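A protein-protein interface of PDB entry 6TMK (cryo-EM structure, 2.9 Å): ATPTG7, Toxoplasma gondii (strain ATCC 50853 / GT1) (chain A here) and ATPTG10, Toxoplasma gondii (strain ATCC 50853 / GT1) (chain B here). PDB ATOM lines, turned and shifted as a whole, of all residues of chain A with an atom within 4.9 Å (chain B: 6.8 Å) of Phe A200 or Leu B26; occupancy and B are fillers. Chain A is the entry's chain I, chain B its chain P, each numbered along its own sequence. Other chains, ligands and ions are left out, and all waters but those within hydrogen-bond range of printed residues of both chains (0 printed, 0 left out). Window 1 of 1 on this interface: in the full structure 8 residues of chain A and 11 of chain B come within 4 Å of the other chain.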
ATOM      1  N   TYR A 196     -12.289  -6.086  -3.615  1.00  0.00           N
ATOM      2  CA  TYR A 196     -11.402  -7.232  -3.763  1.00  0.00           C
ATOM      3  C   TYR A 196     -11.274  -7.645  -5.223  1.00  0.00           C
ATOM      4  O   TYR A 196     -10.191  -8.040  -5.671  1.00  0.00           O
ATOM      5  CB  TYR A 196     -11.924  -8.390  -2.925  1.00  0.00           C
ATOM      6  CG  TYR A 196     -11.936  -8.118  -1.445  1.00  0.00           C
ATOM      7  CD1 TYR A 196     -10.765  -7.866  -0.753  1.00  0.00           C
ATOM      8  CD2 TYR A 196     -13.125  -8.107  -0.738  1.00  0.00           C
ATOM      9  CE1 TYR A 196     -10.780  -7.617   0.599  1.00  0.00           C
ATOM     10  CE2 TYR A 196     -13.147  -7.859   0.609  1.00  0.00           C
ATOM     11  CZ  TYR A 196     -11.975  -7.616   1.275  1.00  0.00           C
ATOM     12  OH  TYR A 196     -12.008  -7.368   2.623  1.00  0.00           O
ATOM     13  N   GLY A 197     -12.365  -7.560  -5.979  1.00  0.00           N
ATOM     14  CA  GLY A 197     -12.290  -7.856  -7.396  1.00  0.00           C
ATOM     15  C   GLY A 197     -11.418  -6.871  -8.149  1.00  0.00           C
ATOM     16  O   GLY A 197     -10.634  -7.257  -9.018  1.00  0.00           O
ATOM     17  N   ASP A 198     -11.541  -5.585  -7.824  1.00  0.00           N
ATOM     18  CA  ASP A 198     -10.680  -4.584  -8.439  1.00  0.00           C
ATOM     19  C   ASP A 198      -9.222  -4.802  -8.056  1.00  0.00           C
ATOM     20  O   ASP A 198      -8.320  -4.589  -8.873  1.00  0.00           O
ATOM     21  CB  ASP A 198     -11.143  -3.187  -8.034  1.00  0.00           C
ATOM     22  CG  ASP A 198     -12.508  -2.844  -8.586  1.00  0.00           C
ATOM     23  OD1 ASP A 198     -13.281  -2.165  -7.880  1.00  0.00           O
ATOM     24  OD2 ASP A 198     -12.813  -3.252  -9.725  1.00  0.00           O
ATOM     25  N   SER A 199      -8.971  -5.241  -6.824  1.00  0.00           N
ATOM     26  CA  SER A 199      -7.599  -5.511  -6.408  1.00  0.00           C
ATOM     27  C   SER A 199      -7.020  -6.694  -7.170  1.00  0.00           C
ATOM     28  O   SER A 199      -5.861  -6.658  -7.600  1.00  0.00           O
ATOM     29  CB  SER A 199      -7.547  -5.762  -4.904  1.00  0.00           C
ATOM     30  OG  SER A 199      -7.819  -4.579  -4.183  1.00  0.00           O
ATOM     31  N   PHE A 200      -7.809  -7.755  -7.341  1.00  0.00           N
ATOM     32  CA  PHE A 200      -7.358  -8.880  -8.146  1.00  0.00           C
ATOM     33  C   PHE A 200      -7.102  -8.455  -9.586  1.00  0.00           C
ATOM     34  O   PHE A 200      -6.115  -8.874 -10.197  1.00  0.00           O
ATOM     35  CB  PHE A 200      -8.384 -10.007  -8.113  1.00  0.00           C
ATOM     36  CG  PHE A 200      -7.958 -11.217  -8.876  1.00  0.00           C
ATOM     37  CD1 PHE A 200      -7.176 -12.178  -8.278  1.00  0.00           C
ATOM     38  CD2 PHE A 200      -8.308 -11.379 -10.199  1.00  0.00           C
ATOM     39  CE1 PHE A 200      -6.773 -13.279  -8.973  1.00  0.00           C
ATOM     40  CE2 PHE A 200      -7.898 -12.480 -10.899  1.00  0.00           C
ATOM     41  CZ  PHE A 200      -7.130 -13.429 -10.286  1.00  0.00           C
ATOM     42  N   PHE A 201      -8.004  -7.657 -10.153  1.00  0.00           N
ATOM     43  CA  PHE A 201      -7.812  -7.142 -11.503  1.00  0.00           C
ATOM     44  C   PHE A 201      -6.501  -6.376 -11.620  1.00  0.00           C
ATOM     45  O   PHE A 201      -5.752  -6.544 -12.591  1.00  0.00           O
ATOM     46  CB  PHE A 201      -8.995  -6.256 -11.873  1.00  0.00           C
ATOM     47  CG  PHE A 201      -8.930  -5.705 -13.253  1.00  0.00           C
ATOM     48  CD1 PHE A 201      -9.121  -6.526 -14.341  1.00  0.00           C
ATOM     49  CD2 PHE A 201      -8.692  -4.364 -13.466  1.00  0.00           C
ATOM     50  CE1 PHE A 201      -9.069  -6.028 -15.607  1.00  0.00           C
ATOM     51  CE2 PHE A 201      -8.637  -3.863 -14.736  1.00  0.00           C
ATOM     52  CZ  PHE A 201      -8.828  -4.697 -15.807  1.00  0.00           C
ATOM     53  N   GLN A 202      -6.211  -5.523 -10.640  1.00  0.00           N
ATOM     54  CA  GLN A 202      -4.990  -4.731 -10.674  1.00  0.00           C
ATOM     55  C   GLN A 202      -3.763  -5.628 -10.589  1.00  0.00           C
ATOM     56  O   GLN A 202      -2.787  -5.444 -11.327  1.00  0.00           O
ATOM     57  CB  GLN A 202      -5.015  -3.729  -9.526  1.00  0.00           C
ATOM     58  CG  GLN A 202      -3.945  -2.672  -9.566  1.00  0.00           C
ATOM     59  CD  GLN A 202      -4.121  -1.714 -10.718  1.00  0.00           C
ATOM     60  OE1 GLN A 202      -3.189  -1.445 -11.472  1.00  0.00           O
ATOM     61  NE2 GLN A 202      -5.323  -1.193 -10.860  1.00  0.00           N
ATOM     62  N   CYS A 203      -3.791  -6.596  -9.676  1.00  0.00           N
ATOM     63  CA  CYS A 203      -2.691  -7.545  -9.572  1.00  0.00           C
ATOM     64  C   CYS A 203      -2.495  -8.313 -10.872  1.00  0.00           C
ATOM     65  O   CYS A 203      -1.360  -8.571 -11.287  1.00  0.00           O
ATOM     66  CB  CYS A 203      -2.960  -8.506  -8.418  1.00  0.00           C
ATOM     67  SG  CYS A 203      -2.712  -7.805  -6.787  1.00  0.00           S
ATOM     68  N   TYR A 204      -3.591  -8.700 -11.525  1.00  0.00           N
ATOM     69  CA  TYR A 204      -3.494  -9.416 -12.790  1.00  0.00           C
ATOM     70  C   TYR A 204      -2.872  -8.546 -13.870  1.00  0.00           C
ATOM     71  O   TYR A 204      -2.058  -9.021 -14.671  1.00  0.00           O
ATOM     72  CB  TYR A 204      -4.882  -9.898 -13.210  1.00  0.00           C
ATOM     73  CG  TYR A 204      -4.999 -10.238 -14.668  1.00  0.00           C
ATOM     74  CD1 TYR A 204      -4.250 -11.256 -15.222  1.00  0.00           C
ATOM     75  CD2 TYR A 204      -5.851  -9.532 -15.495  1.00  0.00           C
ATOM     76  CE1 TYR A 204      -4.351 -11.565 -16.549  1.00  0.00           C
ATOM     77  CE2 TYR A 204      -5.956  -9.834 -16.821  1.00  0.00           C
ATOM     78  CZ  TYR A 204      -5.201 -10.851 -17.347  1.00  0.00           C
ATOM     79  OH  TYR A 204      -5.301 -11.161 -18.679  1.00  0.00           O
ATOM     80  N   PHE A 208       0.960  -9.765 -10.784  1.00  0.00           N
ATOM     81  CA  PHE A 208       1.123 -10.203  -9.402  1.00  0.00           C
ATOM     82  C   PHE A 208       2.525  -9.888  -8.890  1.00  0.00           C
ATOM     83  O   PHE A 208       3.133 -10.669  -8.157  1.00  0.00           O
ATOM     84  CB  PHE A 208       0.796 -11.688  -9.262  1.00  0.00           C
ATOM     85  CG  PHE A 208      -0.560 -12.048  -9.776  1.00  0.00           C
ATOM     86  CD1 PHE A 208      -1.661 -12.010  -8.949  1.00  0.00           C
ATOM     87  CD2 PHE A 208      -0.736 -12.414 -11.092  1.00  0.00           C
ATOM     88  CE1 PHE A 208      -2.904 -12.330  -9.427  1.00  0.00           C
ATOM     89  CE2 PHE A 208      -1.978 -12.734 -11.569  1.00  0.00           C
ATOM     90  CZ  PHE A 208      -3.063 -12.694 -10.737  1.00  0.00           C
ATOM     91  N   ALA A 218      -5.025 -12.280  -2.228  1.00  0.00           N
ATOM     92  CA  ALA A 218      -5.760 -11.548  -3.253  1.00  0.00           C
ATOM     93  C   ALA A 218      -6.939 -12.354  -3.774  1.00  0.00           C
ATOM     94  O   ALA A 218      -7.957 -11.780  -4.177  1.00  0.00           O
ATOM     95  CB  ALA A 218      -4.824 -11.184  -4.398  1.00  0.00           C
ATOM     96  N   THR A 219      -6.819 -13.678  -3.779  1.00  0.00           N
ATOM     97  CA  THR A 219      -7.881 -14.568  -4.223  1.00  0.00           C
ATOM     98  C   THR A 219      -8.766 -15.016  -3.069  1.00  0.00           C
ATOM     99  O   THR A 219      -9.998 -15.077  -3.210  1.00  0.00           O
ATOM    100  CB  THR A 219      -7.254 -15.782  -4.904  1.00  0.00           C
ATOM    101  OG1 THR A 219      -6.192 -15.347  -5.761  1.00  0.00           O
ATOM    102  CG2 THR A 219      -8.272 -16.537  -5.714  1.00  0.00           C
ATOM    103  N   LEU A 222     -11.458 -12.455  -1.908  1.00  0.00           N
ATOM    104  CA  LEU A 222     -12.601 -12.398  -2.805  1.00  0.00           C
ATOM    105  C   LEU A 222     -13.506 -13.608  -2.615  1.00  0.00           C
ATOM    106  O   LEU A 222     -14.735 -13.478  -2.511  1.00  0.00           O
ATOM    107  CB  LEU A 222     -12.096 -12.310  -4.240  1.00  0.00           C
ATOM    108  CG  LEU A 222     -13.097 -12.181  -5.379  1.00  0.00           C
ATOM    109  CD1 LEU A 222     -14.032 -11.013  -5.159  1.00  0.00           C
ATOM    110  CD2 LEU A 222     -12.338 -12.023  -6.658  1.00  0.00           C
ATOM    111  N   ARG B  21     -11.904 -21.684 -11.572  1.00  0.00           N
ATOM    112  CA  ARG B  21     -11.216 -21.946 -12.827  1.00  0.00           C
ATOM    113  C   ARG B  21     -10.947 -20.662 -13.595  1.00  0.00           C
ATOM    114  O   ARG B  21      -9.906 -20.542 -14.247  1.00  0.00           O
ATOM    115  CB  ARG B  21     -12.044 -22.918 -13.657  1.00  0.00           C
ATOM    116  CG  ARG B  21     -11.948 -24.342 -13.164  1.00  0.00           C
ATOM    117  CD  ARG B  21     -13.073 -25.203 -13.693  1.00  0.00           C
ATOM    118  NE  ARG B  21     -13.213 -26.429 -12.914  1.00  0.00           N
ATOM    119  CZ  ARG B  21     -14.234 -27.271 -13.023  1.00  0.00           C
ATOM    120  NH1 ARG B  21     -15.213 -27.026 -13.880  1.00  0.00           N
ATOM    121  NH2 ARG B  21     -14.276 -28.358 -12.270  1.00  0.00           N
ATOM    122  N   LEU B  22     -11.850 -19.688 -13.513  1.00  0.00           N
ATOM    123  CA  LEU B  22     -11.598 -18.391 -14.129  1.00  0.00           C
ATOM    124  C   LEU B  22     -10.347 -17.741 -13.551  1.00  0.00           C
ATOM    125  O   LEU B  22      -9.438 -17.332 -14.289  1.00  0.00           O
ATOM    126  CB  LEU B  22     -12.814 -17.495 -13.924  1.00  0.00           C
ATOM    127  CG  LEU B  22     -12.728 -16.056 -14.405  1.00  0.00           C
ATOM    128  CD1 LEU B  22     -12.725 -15.996 -15.907  1.00  0.00           C
ATOM    129  CD2 LEU B  22     -13.884 -15.278 -13.836  1.00  0.00           C
ATOM    130  N   LEU B  23     -10.297 -17.618 -12.224  1.00  0.00           N
ATOM    131  CA  LEU B  23      -9.147 -16.979 -11.597  1.00  0.00           C
ATOM    132  C   LEU B  23      -7.863 -17.750 -11.878  1.00  0.00           C
ATOM    133  O   LEU B  23      -6.803 -17.148 -12.101  1.00  0.00           O
ATOM    134  CB  LEU B  23      -9.385 -16.852 -10.095  1.00  0.00           C
ATOM    135  CG  LEU B  23     -10.650 -16.102  -9.675  1.00  0.00           C
ATOM    136  CD1 LEU B  23     -10.729 -16.013  -8.178  1.00  0.00           C
ATOM    137  CD2 LEU B  23     -10.703 -14.716 -10.263  1.00  0.00           C
ATOM    138  N   GLY B  24      -7.935 -19.081 -11.883  1.00  0.00           N
ATOM    139  CA  GLY B  24      -6.761 -19.869 -12.210  1.00  0.00           C
ATOM    140  C   GLY B  24      -6.270 -19.630 -13.624  1.00  0.00           C
ATOM    141  O   GLY B  24      -5.067 -19.499 -13.861  1.00  0.00           O
ATOM    142  N   ASP B  25      -7.194 -19.585 -14.583  1.00  0.00           N
ATOM    143  CA  ASP B  25      -6.824 -19.290 -15.961  1.00  0.00           C
ATOM    144  C   ASP B  25      -6.131 -17.941 -16.064  1.00  0.00           C
ATOM    145  O   ASP B  25      -5.124 -17.801 -16.770  1.00  0.00           O
ATOM    146  CB  ASP B  25      -8.062 -19.333 -16.851  1.00  0.00           C
ATOM    147  CG  ASP B  25      -8.450 -20.746 -17.246  1.00  0.00           C
ATOM    148  OD1 ASP B  25      -7.736 -21.694 -16.860  1.00  0.00           O
ATOM    149  OD2 ASP B  25      -9.468 -20.907 -17.952  1.00  0.00           O
ATOM    150  N   LEU B  26      -6.666 -16.928 -15.385  1.00  0.00           N
ATOM    151  CA  LEU B  26      -6.049 -15.607 -15.450  1.00  0.00           C
ATOM    152  C   LEU B  26      -4.645 -15.626 -14.859  1.00  0.00           C
ATOM    153  O   LEU B  26      -3.708 -15.042 -15.428  1.00  0.00           O
ATOM    154  CB  LEU B  26      -6.923 -14.589 -14.729  1.00  0.00           C
ATOM    155  CG  LEU B  26      -8.311 -14.400 -15.321  1.00  0.00           C
ATOM    156  CD1 LEU B  26      -9.145 -13.532 -14.426  1.00  0.00           C
ATOM    157  CD2 LEU B  26      -8.214 -13.787 -16.685  1.00  0.00           C
ATOM    158  N   LYS B  27      -4.475 -16.296 -13.720  1.00  0.00           N
ATOM    159  CA  LYS B  27      -3.150 -16.406 -13.125  1.00  0.00           C
ATOM    160  C   LYS B  27      -2.180 -17.093 -14.072  1.00  0.00           C
ATOM    161  O   LYS B  27      -1.020 -16.685 -14.190  1.00  0.00           O
ATOM    162  CB  LYS B  27      -3.221 -17.176 -11.812  1.00  0.00           C
ATOM    163  CG  LYS B  27      -3.889 -16.448 -10.690  1.00  0.00           C
ATOM    164  CD  LYS B  27      -3.764 -17.228  -9.419  1.00  0.00           C
ATOM    165  CE  LYS B  27      -4.631 -16.656  -8.343  1.00  0.00           C
ATOM    166  NZ  LYS B  27      -5.595 -17.668  -7.864  1.00  0.00           N
ATOM    167  N   LEU B  28      -2.638 -18.138 -14.759  1.00  0.00           N
ATOM    168  CA  LEU B  28      -1.749 -18.875 -15.648  1.00  0.00           C
ATOM    169  C   LEU B  28      -1.390 -18.067 -16.884  1.00  0.00           C
ATOM    170  O   LEU B  28      -0.265 -18.168 -17.382  1.00  0.00           O
ATOM    171  CB  LEU B  28      -2.397 -20.192 -16.049  1.00  0.00           C
ATOM    172  CG  LEU B  28      -2.602 -21.172 -14.901  1.00  0.00           C
ATOM    173  CD1 LEU B  28      -3.575 -22.248 -15.289  1.00  0.00           C
ATOM    174  CD2 LEU B  28      -1.290 -21.774 -14.500  1.00  0.00           C
ATOM    175  N   LEU B  29      -2.316 -17.251 -17.381  1.00  0.00           N
ATOM    176  CA  LEU B  29      -1.982 -16.350 -18.478  1.00  0.00           C
ATOM    177  C   LEU B  29      -0.916 -15.349 -18.054  1.00  0.00           C
ATOM    178  O   LEU B  29       0.062 -15.107 -18.780  1.00  0.00           O
ATOM    179  CB  LEU B  29      -3.237 -15.618 -18.941  1.00  0.00           C
ATOM    180  CG  LEU B  29      -4.328 -16.442 -19.613  1.00  0.00           C
ATOM    181  CD1 LEU B  29      -5.559 -15.592 -19.822  1.00  0.00           C
ATOM    182  CD2 LEU B  29      -3.845 -16.993 -20.923  1.00  0.00           C
ATOM    183  N   ALA B  30      -1.095 -14.748 -16.878  1.00  0.00           N
ATOM    184  CA  ALA B  30      -0.085 -13.832 -16.363  1.00  0.00           C
ATOM    185  C   ALA B  30       1.265 -14.521 -16.214  1.00  0.00           C
ATOM    186  O   ALA B  30       2.310 -13.940 -16.535  1.00  0.00           O
ATOM    187  CB  ALA B  30      -0.545 -13.260 -15.027  1.00  0.00           C
ATOM    188  N   ALA B  31       1.263 -15.766 -15.736  1.00  0.00           N
ATOM    189  CA  ALA B  31       2.509 -16.504 -15.573  1.00  0.00           C
ATOM    190  C   ALA B  31       3.174 -16.775 -16.913  1.00  0.00           C
ATOM    191  O   ALA B  31       4.398 -16.681 -17.034  1.00  0.00           O
ATOM    192  CB  ALA B  31       2.245 -17.810 -14.835  1.00  0.00           C
ATOM    193  N   LEU B  51      -3.584 -25.489 -17.794  1.00  0.00           N
ATOM    194  CA  LEU B  51      -4.668 -24.565 -18.125  1.00  0.00           C
ATOM    195  C   LEU B  51      -5.967 -25.306 -18.435  1.00  0.00           C
ATOM    196  O   LEU B  51      -6.519 -25.223 -19.529  1.00  0.00           O
ATOM    197  CB  LEU B  51      -4.258 -23.682 -19.295  1.00  0.00           C
ATOM    198  CG  LEU B  51      -5.185 -22.505 -19.562  1.00  0.00           C
ATOM    199  CD1 LEU B  51      -4.837 -21.350 -18.659  1.00  0.00           C
ATOM    200  CD2 LEU B  51      -5.098 -22.096 -21.001  1.00  0.00           C
ATOM    201  N   LEU B  83     -10.087  -8.292 -20.536  1.00  0.00           N
ATOM    202  CA  LEU B  83      -9.155  -9.111 -19.767  1.00  0.00           C
ATOM    203  C   LEU B  83      -7.786  -9.197 -20.432  1.00  0.00           C
ATOM    204  O   LEU B  83      -6.767  -9.284 -19.738  1.00  0.00           O
ATOM    205  CB  LEU B  83      -9.724 -10.513 -19.569  1.00  0.00           C
ATOM    206  CG  LEU B  83     -11.087 -10.606 -18.894  1.00  0.00           C
ATOM    207  CD1 LEU B  83     -11.506 -12.050 -18.808  1.00  0.00           C
ATOM    208  CD2 LEU B  83     -11.061  -9.978 -17.525  1.00  0.00           C
ATOM    209  N   CYS B  84      -7.742  -9.169 -21.760  1.00  0.00           N
ATOM    210  CA  CYS B  84      -6.524  -9.459 -22.516  1.00  0.00           C
ATOM    211  C   CYS B  84      -6.553  -8.667 -23.813  1.00  0.00           C
ATOM    212  O   CYS B  84      -6.848  -9.203 -24.886  1.00  0.00           O
ATOM    213  CB  CYS B  84      -6.405 -10.954 -22.807  1.00  0.00           C
ATOM    214  SG  CYS B  84      -6.196 -12.017 -21.371  1.00  0.00           S
ATOM    215  N   MET B 102     -10.048 -19.235 -23.371  1.00  0.00           N
ATOM    216  CA  MET B 102     -10.622 -18.190 -22.535  1.00  0.00           C
ATOM    217  C   MET B 102     -11.915 -17.659 -23.137  1.00  0.00           C
ATOM    218  O   MET B 102     -12.902 -17.431 -22.422  1.00  0.00           O
ATOM    219  CB  MET B 102      -9.603 -17.068 -22.350  1.00  0.00           C
ATOM    220  CG  MET B 102     -10.125 -15.849 -21.624  1.00  0.00           C
ATOM    221  SD  MET B 102     -11.119 -16.226 -20.169  1.00  0.00           S
ATOM    222  CE  MET B 102      -9.888 -16.960 -19.104  1.00  0.00           C
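NZ of Lys B27 is in hydrogen-bond range of OG1 of Thr A219.
O of Leu B83 is in hydrogen-bond range of OH of Tyr A204 (2.6 Å).
The side-chain sulfur of Cys B84 sits at hydrogen-bond distance from the side-chain hydroxyl of Tyr A204 (3.0 Å).
O of Cys A203 is in hydrogen-bond range of N of Phe A208.
Among the printed residues, merely in contact across the chains: Phe A200 with Leu B23 (3.6 Å), Phe A200 with Leu B26 (3.9 Å), Tyr A204 with Leu B26 (3.7 Å), Phe A208 with Lys B27 (3.8 Å), Phe A208 with Ala B30 (3.8 Å) and Thr A219 with Leu B23 (3.5 Å).
Of chain B, only Leu B23 and Leu B26 come within 4 Å of Phe A200.
Printed residues of chain A within 4 Å of Leu B26: Phe A200 (3.9 Å) and Tyr A204 (3.7 Å).
Of the printed residues of chain B, Phe A208 touches Lys B27 and Ala B30.
Of the printed residues of chain A, Ala B30 touches Phe A208.
Printed residues of chain A within 4 Å of Leu B23: Phe A200 (3.6 Å) and Thr A219 (3.5 Å).
Gly B24 touches none of the printed residues of chain A.
Met B102 touches none of the printed residues of chain A.
The nearest residue of chain B that does not touch Phe A200 is Lys B27 (4.05 Å).
The nearest printed residue of chain A that does not touch Cys B84 is Phe A201 (7.0 Å).
Of the 15 printed residues of chain B, 6 touch a printed residue of chain A.
Printed residues of chain B that touch a printed residue of chain A: Leu B23, Leu B26, Lys B27, Ala B30, Leu B83 and Cys B84.
Of the 13 printed residues of chain A, 4 touch a printed residue of chain B.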
